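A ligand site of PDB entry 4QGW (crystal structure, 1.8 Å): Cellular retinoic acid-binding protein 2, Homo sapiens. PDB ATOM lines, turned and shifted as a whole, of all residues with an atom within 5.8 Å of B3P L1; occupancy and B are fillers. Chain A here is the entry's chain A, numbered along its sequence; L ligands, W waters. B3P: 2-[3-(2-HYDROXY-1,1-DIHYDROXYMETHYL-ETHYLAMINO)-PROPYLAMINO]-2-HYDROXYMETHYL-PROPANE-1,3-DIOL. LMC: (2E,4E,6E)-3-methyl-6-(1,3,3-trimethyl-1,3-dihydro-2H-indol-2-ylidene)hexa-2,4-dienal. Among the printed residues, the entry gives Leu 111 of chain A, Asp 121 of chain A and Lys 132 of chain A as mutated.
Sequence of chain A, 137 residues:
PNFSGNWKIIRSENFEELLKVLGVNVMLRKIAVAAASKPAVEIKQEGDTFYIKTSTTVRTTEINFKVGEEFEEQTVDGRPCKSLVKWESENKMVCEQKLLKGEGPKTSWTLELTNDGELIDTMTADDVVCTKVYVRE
Phe 15 touches B3P L1 (CZ to O1, 3.6 Å). Val 41 touches B3P L1 (CG2 to O6, 3.7 Å). CD1 of Ile 63 touches O5 of B3P L1 (3.3 Å). Val 76 touches B3P L1. Trp 109 touches B3P L1. Leu 111 touches B3P L1 (CG to O4, 3.1 Å). CD of Lys 132 touches O2 of B3P L1 (3.7 Å). Hydrophobic or aromatic side chains that line B3P L1: Phe 15, Val 41, Ile 63, Val 76, Trp 109, Leu 111 and Met 123.
The backbone NH (N) of Asp 121 lies within hydrogen-bond range of the backbone carbonyl oxygen (O) of Lys 132 (2.8 Å). O of Thr 61 is in hydrogen-bond range of N of Thr 54 (2.8 Å). The side-chain carboxylate of Glu 73 lies within hydrogen-bond range of the indole nitrogen of Trp 109 (3.0 Å). The backbone NH (N) of Ile 63 is in hydrogen-bond range of the backbone carbonyl oxygen (O) of Ile 52.
Water W1 lies within hydrogen-bond range of the side-chain hydroxyl of Tyr 134 (2.5 Å), the side-chain carboxylate of Asp 121 (2.6 Å) and an oxygen (O2) of B3P L1 (2.9 Å). Water W5 lies within hydrogen-bond range of OE1 of Glu 73 (2.5 Å) and O5 of B3P L1 (3.3 Å). Water W2 lies within hydrogen-bond range of the side-chain hydroxyl (OG1) of Thr 54 (2.7 Å), the backbone carbonyl oxygen (O) of Ile 52 (3.0 Å) and an oxygen (O5) of B3P L1 (3.3 Å).
The side-chain sulfur (SD) of Met 123 is in hydrogen-bond range of a nitrogen (N2) of B3P L1 (3.6 Å). The side-chain hydroxyl (OG1) of Thr 54 lies within hydrogen-bond range of an oxygen (O6) of B3P L1 (2.7 Å). The side-chain amino group of Lys 132 is bonded to a carbon (C18) of LMC L2 (1.3 Å). N1 of B3P L1 is in salt-bridge range of OD2 of Asp 121 (2.9 Å).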
ATOM      1  N   PHE A  15     -10.316 -14.119  -0.467  1.00  0.00           N
ATOM      2  CA  PHE A  15     -11.681 -14.624  -0.363  1.00  0.00           C
ATOM      3  C   PHE A  15     -11.929 -15.418   0.921  1.00  0.00           C
ATOM      4  O   PHE A  15     -12.972 -15.258   1.569  1.00  0.00           O
ATOM      5  CB  PHE A  15     -12.088 -15.432  -1.595  1.00  0.00           C
ATOM      6  CG  PHE A  15     -13.517 -15.913  -1.570  1.00  0.00           C
ATOM      7  CD1 PHE A  15     -14.579 -15.013  -1.515  1.00  0.00           C
ATOM      8  CD2 PHE A  15     -13.797 -17.263  -1.595  1.00  0.00           C
ATOM      9  CE1 PHE A  15     -15.890 -15.468  -1.489  1.00  0.00           C
ATOM     10  CE2 PHE A  15     -15.097 -17.724  -1.561  1.00  0.00           C
ATOM     11  CZ  PHE A  15     -16.147 -16.818  -1.516  1.00  0.00           C
ATOM     12  N   PRO A  39     -15.845 -19.658  -9.312  1.00  0.00           N
ATOM     13  CA  PRO A  39     -17.041 -19.079  -9.956  1.00  0.00           C
ATOM     14  C   PRO A  39     -16.850 -18.732 -11.431  1.00  0.00           C
ATOM     15  O   PRO A  39     -15.774 -18.341 -11.874  1.00  0.00           O
ATOM     16  CB  PRO A  39     -17.293 -17.802  -9.140  1.00  0.00           C
ATOM     17  CG  PRO A  39     -15.922 -17.395  -8.658  1.00  0.00           C
ATOM     18  CD  PRO A  39     -15.171 -18.695  -8.420  1.00  0.00           C
ATOM     19  N   VAL A  41     -19.014 -16.248 -14.178  1.00  0.00           N
ATOM     20  CA  VAL A  41     -20.051 -15.220 -14.150  1.00  0.00           C
ATOM     21  C   VAL A  41     -20.559 -14.900 -15.553  1.00  0.00           C
ATOM     22  O   VAL A  41     -19.793 -14.528 -16.445  1.00  0.00           O
ATOM     23  CB  VAL A  41     -19.528 -13.911 -13.485  1.00  0.00           C
ATOM     24  CG1 VAL A  41     -20.574 -12.804 -13.574  1.00  0.00           C
ATOM     25  CG2 VAL A  41     -19.151 -14.178 -12.024  1.00  0.00           C
ATOM     26  N   ILE A  52     -27.315 -11.231 -13.863  1.00  0.00           N
ATOM     27  CA  ILE A  52     -26.009 -11.793 -13.526  1.00  0.00           C
ATOM     28  C   ILE A  52     -26.167 -13.181 -12.946  1.00  0.00           C
ATOM     29  O   ILE A  52     -26.793 -13.376 -11.900  1.00  0.00           O
ATOM     30  CB  ILE A  52     -25.228 -10.893 -12.527  1.00  0.00           C
ATOM     31  CG1 ILE A  52     -25.108  -9.475 -13.087  1.00  0.00           C
ATOM     32  CG2 ILE A  52     -23.842 -11.463 -12.275  1.00  0.00           C
ATOM     33  CD1 ILE A  52     -24.422  -8.470 -12.136  1.00  0.00           C
ATOM     34  N   THR A  54     -24.159 -16.401 -11.447  1.00  0.00           N
ATOM     35  CA  THR A  54     -22.892 -16.845 -10.896  1.00  0.00           C
ATOM     36  C   THR A  54     -22.976 -18.335 -10.614  1.00  0.00           C
ATOM     37  O   THR A  54     -23.797 -18.782  -9.793  1.00  0.00           O
ATOM     38  CB  THR A  54     -22.538 -16.065  -9.591  1.00  0.00           C
ATOM     39  OG1 THR A  54     -22.452 -14.654  -9.890  1.00  0.00           O
ATOM     40  CG2 THR A  54     -21.196 -16.529  -9.022  1.00  0.00           C
ATOM     41  N   THR A  61     -26.632 -19.294  -9.125  1.00  0.00           N
ATOM     42  CA  THR A  61     -27.469 -18.234  -8.560  1.00  0.00           C
ATOM     43  C   THR A  61     -27.611 -17.112  -9.582  1.00  0.00           C
ATOM     44  O   THR A  61     -26.641 -16.733 -10.261  1.00  0.00           O
ATOM     45  CB  THR A  61     -26.929 -17.688  -7.214  1.00  0.00           C
ATOM     46  OG1 THR A  61     -25.573 -17.262  -7.376  1.00  0.00           O
ATOM     47  CG2 THR A  61     -26.991 -18.741  -6.132  1.00  0.00           C
ATOM     48  N   ILE A  63     -29.105 -13.188 -10.254  1.00  0.00           N
ATOM     49  CA  ILE A  63     -29.763 -11.949  -9.858  1.00  0.00           C
ATOM     50  C   ILE A  63     -30.232 -11.118 -11.045  1.00  0.00           C
ATOM     51  O   ILE A  63     -29.590 -11.092 -12.098  1.00  0.00           O
ATOM     52  CB  ILE A  63     -28.923 -11.062  -8.921  1.00  0.00           C
ATOM     53  CG1 ILE A  63     -27.612 -10.632  -9.580  1.00  0.00           C
ATOM     54  CG2 ILE A  63     -28.682 -11.777  -7.588  1.00  0.00           C
ATOM     55  CD1 ILE A  63     -26.909  -9.520  -8.794  1.00  0.00           C
ATOM     56  N   GLU A  73     -31.385 -10.220  -2.731  1.00  0.00           N
ATOM     57  CA  GLU A  73     -30.405 -11.258  -3.032  1.00  0.00           C
ATOM     58  C   GLU A  73     -29.929 -11.825  -1.708  1.00  0.00           C
ATOM     59  O   GLU A  73     -30.657 -11.773  -0.710  1.00  0.00           O
ATOM     60  CB  GLU A  73     -29.251 -10.693  -3.869  1.00  0.00           C
ATOM     61  CG  GLU A  73     -28.531  -9.499  -3.243  1.00  0.00           C
ATOM     62  CD  GLU A  73     -27.222  -9.151  -3.971  1.00  0.00           C
ATOM     63  OE1 GLU A  73     -26.740  -9.994  -4.765  1.00  0.00           O
ATOM     64  OE2 GLU A  73     -26.677  -8.044  -3.753  1.00  0.00           O
ATOM     65  N   VAL A  76     -22.794 -12.764   0.922  1.00  0.00           N
ATOM     66  CA  VAL A  76     -21.840 -13.793   0.492  1.00  0.00           C
ATOM     67  C   VAL A  76     -22.051 -15.059   1.311  1.00  0.00           C
ATOM     68  O   VAL A  76     -21.995 -16.176   0.780  1.00  0.00           O
ATOM     69  CB  VAL A  76     -20.374 -13.290   0.581  1.00  0.00           C
ATOM     70  CG1 VAL A  76     -19.385 -14.422   0.331  1.00  0.00           C
ATOM     71  CG2 VAL A  76     -20.141 -12.149  -0.412  1.00  0.00           C
ATOM     72  N   SER A 108     -20.969  -4.990   1.093  1.00  0.00           N
ATOM     73  CA  SER A 108     -21.227  -4.300  -0.160  1.00  0.00           C
ATOM     74  C   SER A 108     -20.457  -5.031  -1.245  1.00  0.00           C
ATOM     75  O   SER A 108     -19.631  -5.895  -0.964  1.00  0.00           O
ATOM     76  CB  SER A 108     -20.723  -2.852  -0.081  1.00  0.00           C
ATOM     77  OG  SER A 108     -19.307  -2.814  -0.013  1.00  0.00           O
ATOM     78  N   TRP A 109     -20.751  -4.679  -2.493  1.00  0.00           N
ATOM     79  CA  TRP A 109     -19.916  -5.142  -3.601  1.00  0.00           C
ATOM     80  C   TRP A 109     -19.839  -4.094  -4.707  1.00  0.00           C
ATOM     81  O   TRP A 109     -20.712  -3.240  -4.819  1.00  0.00           O
ATOM     82  CB  TRP A 109     -20.370  -6.506  -4.142  1.00  0.00           C
ATOM     83  CG  TRP A 109     -21.806  -6.657  -4.633  1.00  0.00           C
ATOM     84  CD1 TRP A 109     -22.849  -7.204  -3.950  1.00  0.00           C
ATOM     85  CD2 TRP A 109     -22.313  -6.319  -5.930  1.00  0.00           C
ATOM     86  NE1 TRP A 109     -23.981  -7.216  -4.728  1.00  0.00           N
ATOM     87  CE2 TRP A 109     -23.687  -6.675  -5.947  1.00  0.00           C
ATOM     88  CE3 TRP A 109     -21.756  -5.727  -7.069  1.00  0.00           C
ATOM     89  CZ2 TRP A 109     -24.498  -6.472  -7.059  1.00  0.00           C
ATOM     90  CZ3 TRP A 109     -22.561  -5.517  -8.170  1.00  0.00           C
ATOM     91  CH2 TRP A 109     -23.927  -5.892  -8.161  1.00  0.00           C
ATOM     92  N   THR A 110     -18.768  -4.135  -5.498  1.00  0.00           N
ATOM     93  CA  THR A 110     -18.644  -3.247  -6.633  1.00  0.00           C
ATOM     94  C   THR A 110     -18.238  -4.069  -7.846  1.00  0.00           C
ATOM     95  O   THR A 110     -17.546  -5.080  -7.714  1.00  0.00           O
ATOM     96  CB  THR A 110     -17.579  -2.142  -6.398  1.00  0.00           C
ATOM     97  OG1 THR A 110     -16.282  -2.744  -6.306  1.00  0.00           O
ATOM     98  CG2 THR A 110     -17.872  -1.405  -5.104  1.00  0.00           C
ATOM     99  N   LEU A 111     -18.678  -3.637  -9.008  1.00  0.00           N
ATOM    100  CA  LEU A 111     -18.241  -4.253 -10.253  1.00  0.00           C
ATOM    101  C   LEU A 111     -17.764  -3.143 -11.159  1.00  0.00           C
ATOM    102  O   LEU A 111     -18.465  -2.140 -11.364  1.00  0.00           O
ATOM    103  CB  LEU A 111     -19.393  -4.954 -10.968  1.00  0.00           C
ATOM    104  CG  LEU A 111     -19.743  -6.415 -10.750  1.00  0.00           C
ATOM    105  CD1 LEU A 111     -20.832  -6.822 -11.751  1.00  0.00           C
ATOM    106  CD2 LEU A 111     -18.515  -7.314 -10.887  1.00  0.00           C
ATOM    107  N   ASP A 121     -14.465  -7.494  -9.556  1.00  0.00           N
ATOM    108  CA  ASP A 121     -15.527  -7.636  -8.568  1.00  0.00           C
ATOM    109  C   ASP A 121     -14.907  -7.484  -7.192  1.00  0.00           C
ATOM    110  O   ASP A 121     -14.033  -8.242  -6.792  1.00  0.00           O
ATOM    111  CB  ASP A 121     -16.149  -9.025  -8.692  1.00  0.00           C
ATOM    112  CG  ASP A 121     -17.418  -9.195  -7.839  1.00  0.00           C
ATOM    113  OD1 ASP A 121     -17.988  -8.194  -7.329  1.00  0.00           O
ATOM    114  OD2 ASP A 121     -17.898 -10.351  -7.725  1.00  0.00           O
ATOM    115  N   THR A 122     -15.338  -6.479  -6.442  1.00  0.00           N
ATOM    116  CA  THR A 122     -14.834  -6.293  -5.096  1.00  0.00           C
ATOM    117  C   THR A 122     -15.962  -6.506  -4.084  1.00  0.00           C
ATOM    118  O   THR A 122     -17.070  -6.006  -4.273  1.00  0.00           O
ATOM    119  CB  THR A 122     -14.223  -4.890  -4.947  1.00  0.00           C
ATOM    120  OG1 THR A 122     -12.994  -4.831  -5.675  1.00  0.00           O
ATOM    121  CG2 THR A 122     -13.984  -4.573  -3.499  1.00  0.00           C
ATOM    122  N   MET A 123     -15.676  -7.252  -3.031  1.00  0.00           N
ATOM    123  CA  MET A 123     -16.626  -7.523  -1.972  1.00  0.00           C
ATOM    124  C   MET A 123     -16.020  -7.055  -0.661  1.00  0.00           C
ATOM    125  O   MET A 123     -14.825  -7.276  -0.424  1.00  0.00           O
ATOM    126  CB  MET A 123     -16.906  -9.018  -1.872  1.00  0.00           C
ATOM    127  CG  MET A 123     -17.566  -9.630  -3.093  1.00  0.00           C
ATOM    128  SD  MET A 123     -16.880 -11.241  -3.571  1.00  0.00           S
ATOM    129  CE  MET A 123     -15.505 -10.703  -4.586  1.00  0.00           C
ATOM    130  N   LYS A 132     -11.883 -10.085  -6.946  1.00  0.00           N
ATOM    131  CA  LYS A 132     -11.815 -11.101  -7.993  1.00  0.00           C
ATOM    132  C   LYS A 132     -11.769 -10.405  -9.334  1.00  0.00           C
ATOM    133  O   LYS A 132     -12.431  -9.387  -9.551  1.00  0.00           O
ATOM    134  CB  LYS A 132     -13.008 -12.060  -7.872  1.00  0.00           C
ATOM    135  CG  LYS A 132     -12.933 -12.902  -6.618  1.00  0.00           C
ATOM    136  CD  LYS A 132     -14.212 -13.710  -6.413  1.00  0.00           C
ATOM    137  CE  LYS A 132     -14.122 -14.467  -5.092  1.00  0.00           C
ATOM    138  NZ  LYS A 132     -13.299 -15.691  -5.258  1.00  0.00           N
ATOM    139  N   TYR A 134     -11.951 -11.033 -13.584  1.00  0.00           N
ATOM    140  CA  TYR A 134     -12.379 -11.934 -14.648  1.00  0.00           C
ATOM    141  C   TYR A 134     -12.010 -11.378 -16.018  1.00  0.00           C
ATOM    142  O   TYR A 134     -11.837 -10.173 -16.176  1.00  0.00           O
ATOM    143  CB  TYR A 134     -13.895 -12.089 -14.636  1.00  0.00           C
ATOM    144  CG  TYR A 134     -14.480 -12.639 -13.361  1.00  0.00           C
ATOM    145  CD1 TYR A 134     -14.635 -11.828 -12.233  1.00  0.00           C
ATOM    146  CD2 TYR A 134     -14.898 -13.951 -13.278  1.00  0.00           C
ATOM    147  CE1 TYR A 134     -15.197 -12.330 -11.065  1.00  0.00           C
ATOM    148  CE2 TYR A 134     -15.446 -14.473 -12.105  1.00  0.00           C
ATOM    149  CZ  TYR A 134     -15.590 -13.653 -10.997  1.00  0.00           C
ATOM    150  OH  TYR A 134     -16.149 -14.166  -9.842  1.00  0.00           O
HETATM  151  C1  B3P L   1     -20.534 -10.313  -4.577  1.00  0.00           C
HETATM  152  C2  B3P L   1     -20.731 -11.806  -4.323  1.00  0.00           C
HETATM  153  C3  B3P L   1     -21.093  -9.870  -5.927  1.00  0.00           C
HETATM  154  N1  B3P L   1     -20.683 -10.731  -7.036  1.00  0.00           N
HETATM  155  C4  B3P L   1     -21.535 -10.834  -8.187  1.00  0.00           C
HETATM  156  C5  B3P L   1     -21.807  -9.434  -8.712  1.00  0.00           C
HETATM  157  C6  B3P L   1     -22.839 -11.527  -7.800  1.00  0.00           C
HETATM  158  C7  B3P L   1     -20.792 -11.618  -9.269  1.00  0.00           C
HETATM  159  N2  B3P L   1     -19.855 -12.632  -5.142  1.00  0.00           N
HETATM  160  C8  B3P L   1     -19.838 -14.061  -4.952  1.00  0.00           C
HETATM  161  C9  B3P L   1     -18.992 -14.381  -3.725  1.00  0.00           C
HETATM  162  C10 B3P L   1     -19.250 -14.666  -6.214  1.00  0.00           C
HETATM  163  C11 B3P L   1     -21.284 -14.532  -4.779  1.00  0.00           C
HETATM  164  O1  B3P L   1     -19.052 -15.761  -3.340  1.00  0.00           O
HETATM  165  O2  B3P L   1     -17.821 -14.576  -6.157  1.00  0.00           O
HETATM  166  O3  B3P L   1     -21.877 -14.686  -6.087  1.00  0.00           O
HETATM  167  O4  B3P L   1     -20.545  -8.781  -8.895  1.00  0.00           O
HETATM  168  O5  B3P L   1     -23.943 -10.797  -8.332  1.00  0.00           O
HETATM  169  O6  B3P L   1     -20.617 -12.990  -8.881  1.00  0.00           O
HETATM  170  C18 LMC L   2     -13.854 -16.821  -5.273  1.00  0.00           C
HETATM  171  C17 LMC L   2     -13.032 -18.021  -5.444  1.00  0.00           C
HETATM  172  C16 LMC L   2     -13.509 -19.256  -5.193  1.00  0.00           C
HETATM  173  C20 LMC L   2     -14.926 -19.451  -4.718  1.00  0.00           C
HETATM  174  C15 LMC L   2     -12.622 -20.431  -5.387  1.00  0.00           C
HETATM  175  C14 LMC L   2     -11.474 -20.311  -5.907  1.00  0.00           C
HETATM  176  C13 LMC L   2     -10.451 -21.373  -5.723  1.00  0.00           C
HETATM  177  C8  LMC L   2      -9.377 -21.405  -6.420  1.00  0.00           C
HETATM  178  C7  LMC L   2      -8.990 -20.389  -7.458  1.00  0.00           C
HETATM  179  C11 LMC L   2     -10.010 -20.354  -8.600  1.00  0.00           C
HETATM  180  C10 LMC L   2      -8.788 -19.012  -6.842  1.00  0.00           C
HETATM  181  C2  LMC L   2      -7.696 -20.944  -7.922  1.00  0.00           C
HETATM  182  C3  LMC L   2      -7.432 -22.176  -7.166  1.00  0.00           C
HETATM  183  N9  LMC L   2      -8.455 -22.417  -6.286  1.00  0.00           N
HETATM  184  C12 LMC L   2      -8.542 -23.561  -5.353  1.00  0.00           C
HETATM  185  C1  LMC L   2      -6.920 -20.461  -8.823  1.00  0.00           C
HETATM  186  C6  LMC L   2      -5.822 -21.109  -9.087  1.00  0.00           C
HETATM  187  C5  LMC L   2      -5.465 -22.300  -8.415  1.00  0.00           C
HETATM  188  C4  LMC L   2      -6.272 -22.882  -7.429  1.00  0.00           C
HETATM  189  O   HOH W   1     -17.597 -12.789  -8.412  1.00  0.00           O
HETATM  190  O   HOH W   2     -24.985 -13.687  -9.534  1.00  0.00           O
HETATM  191  O   HOH W   3     -17.281 -16.977  -4.972  1.00  0.00           O
HETATM  192  O   HOH W   4     -24.984 -13.718  -6.905  1.00  0.00           O
HETATM  193  O   HOH W   5     -24.351 -10.712  -5.009  1.00  0.00           O
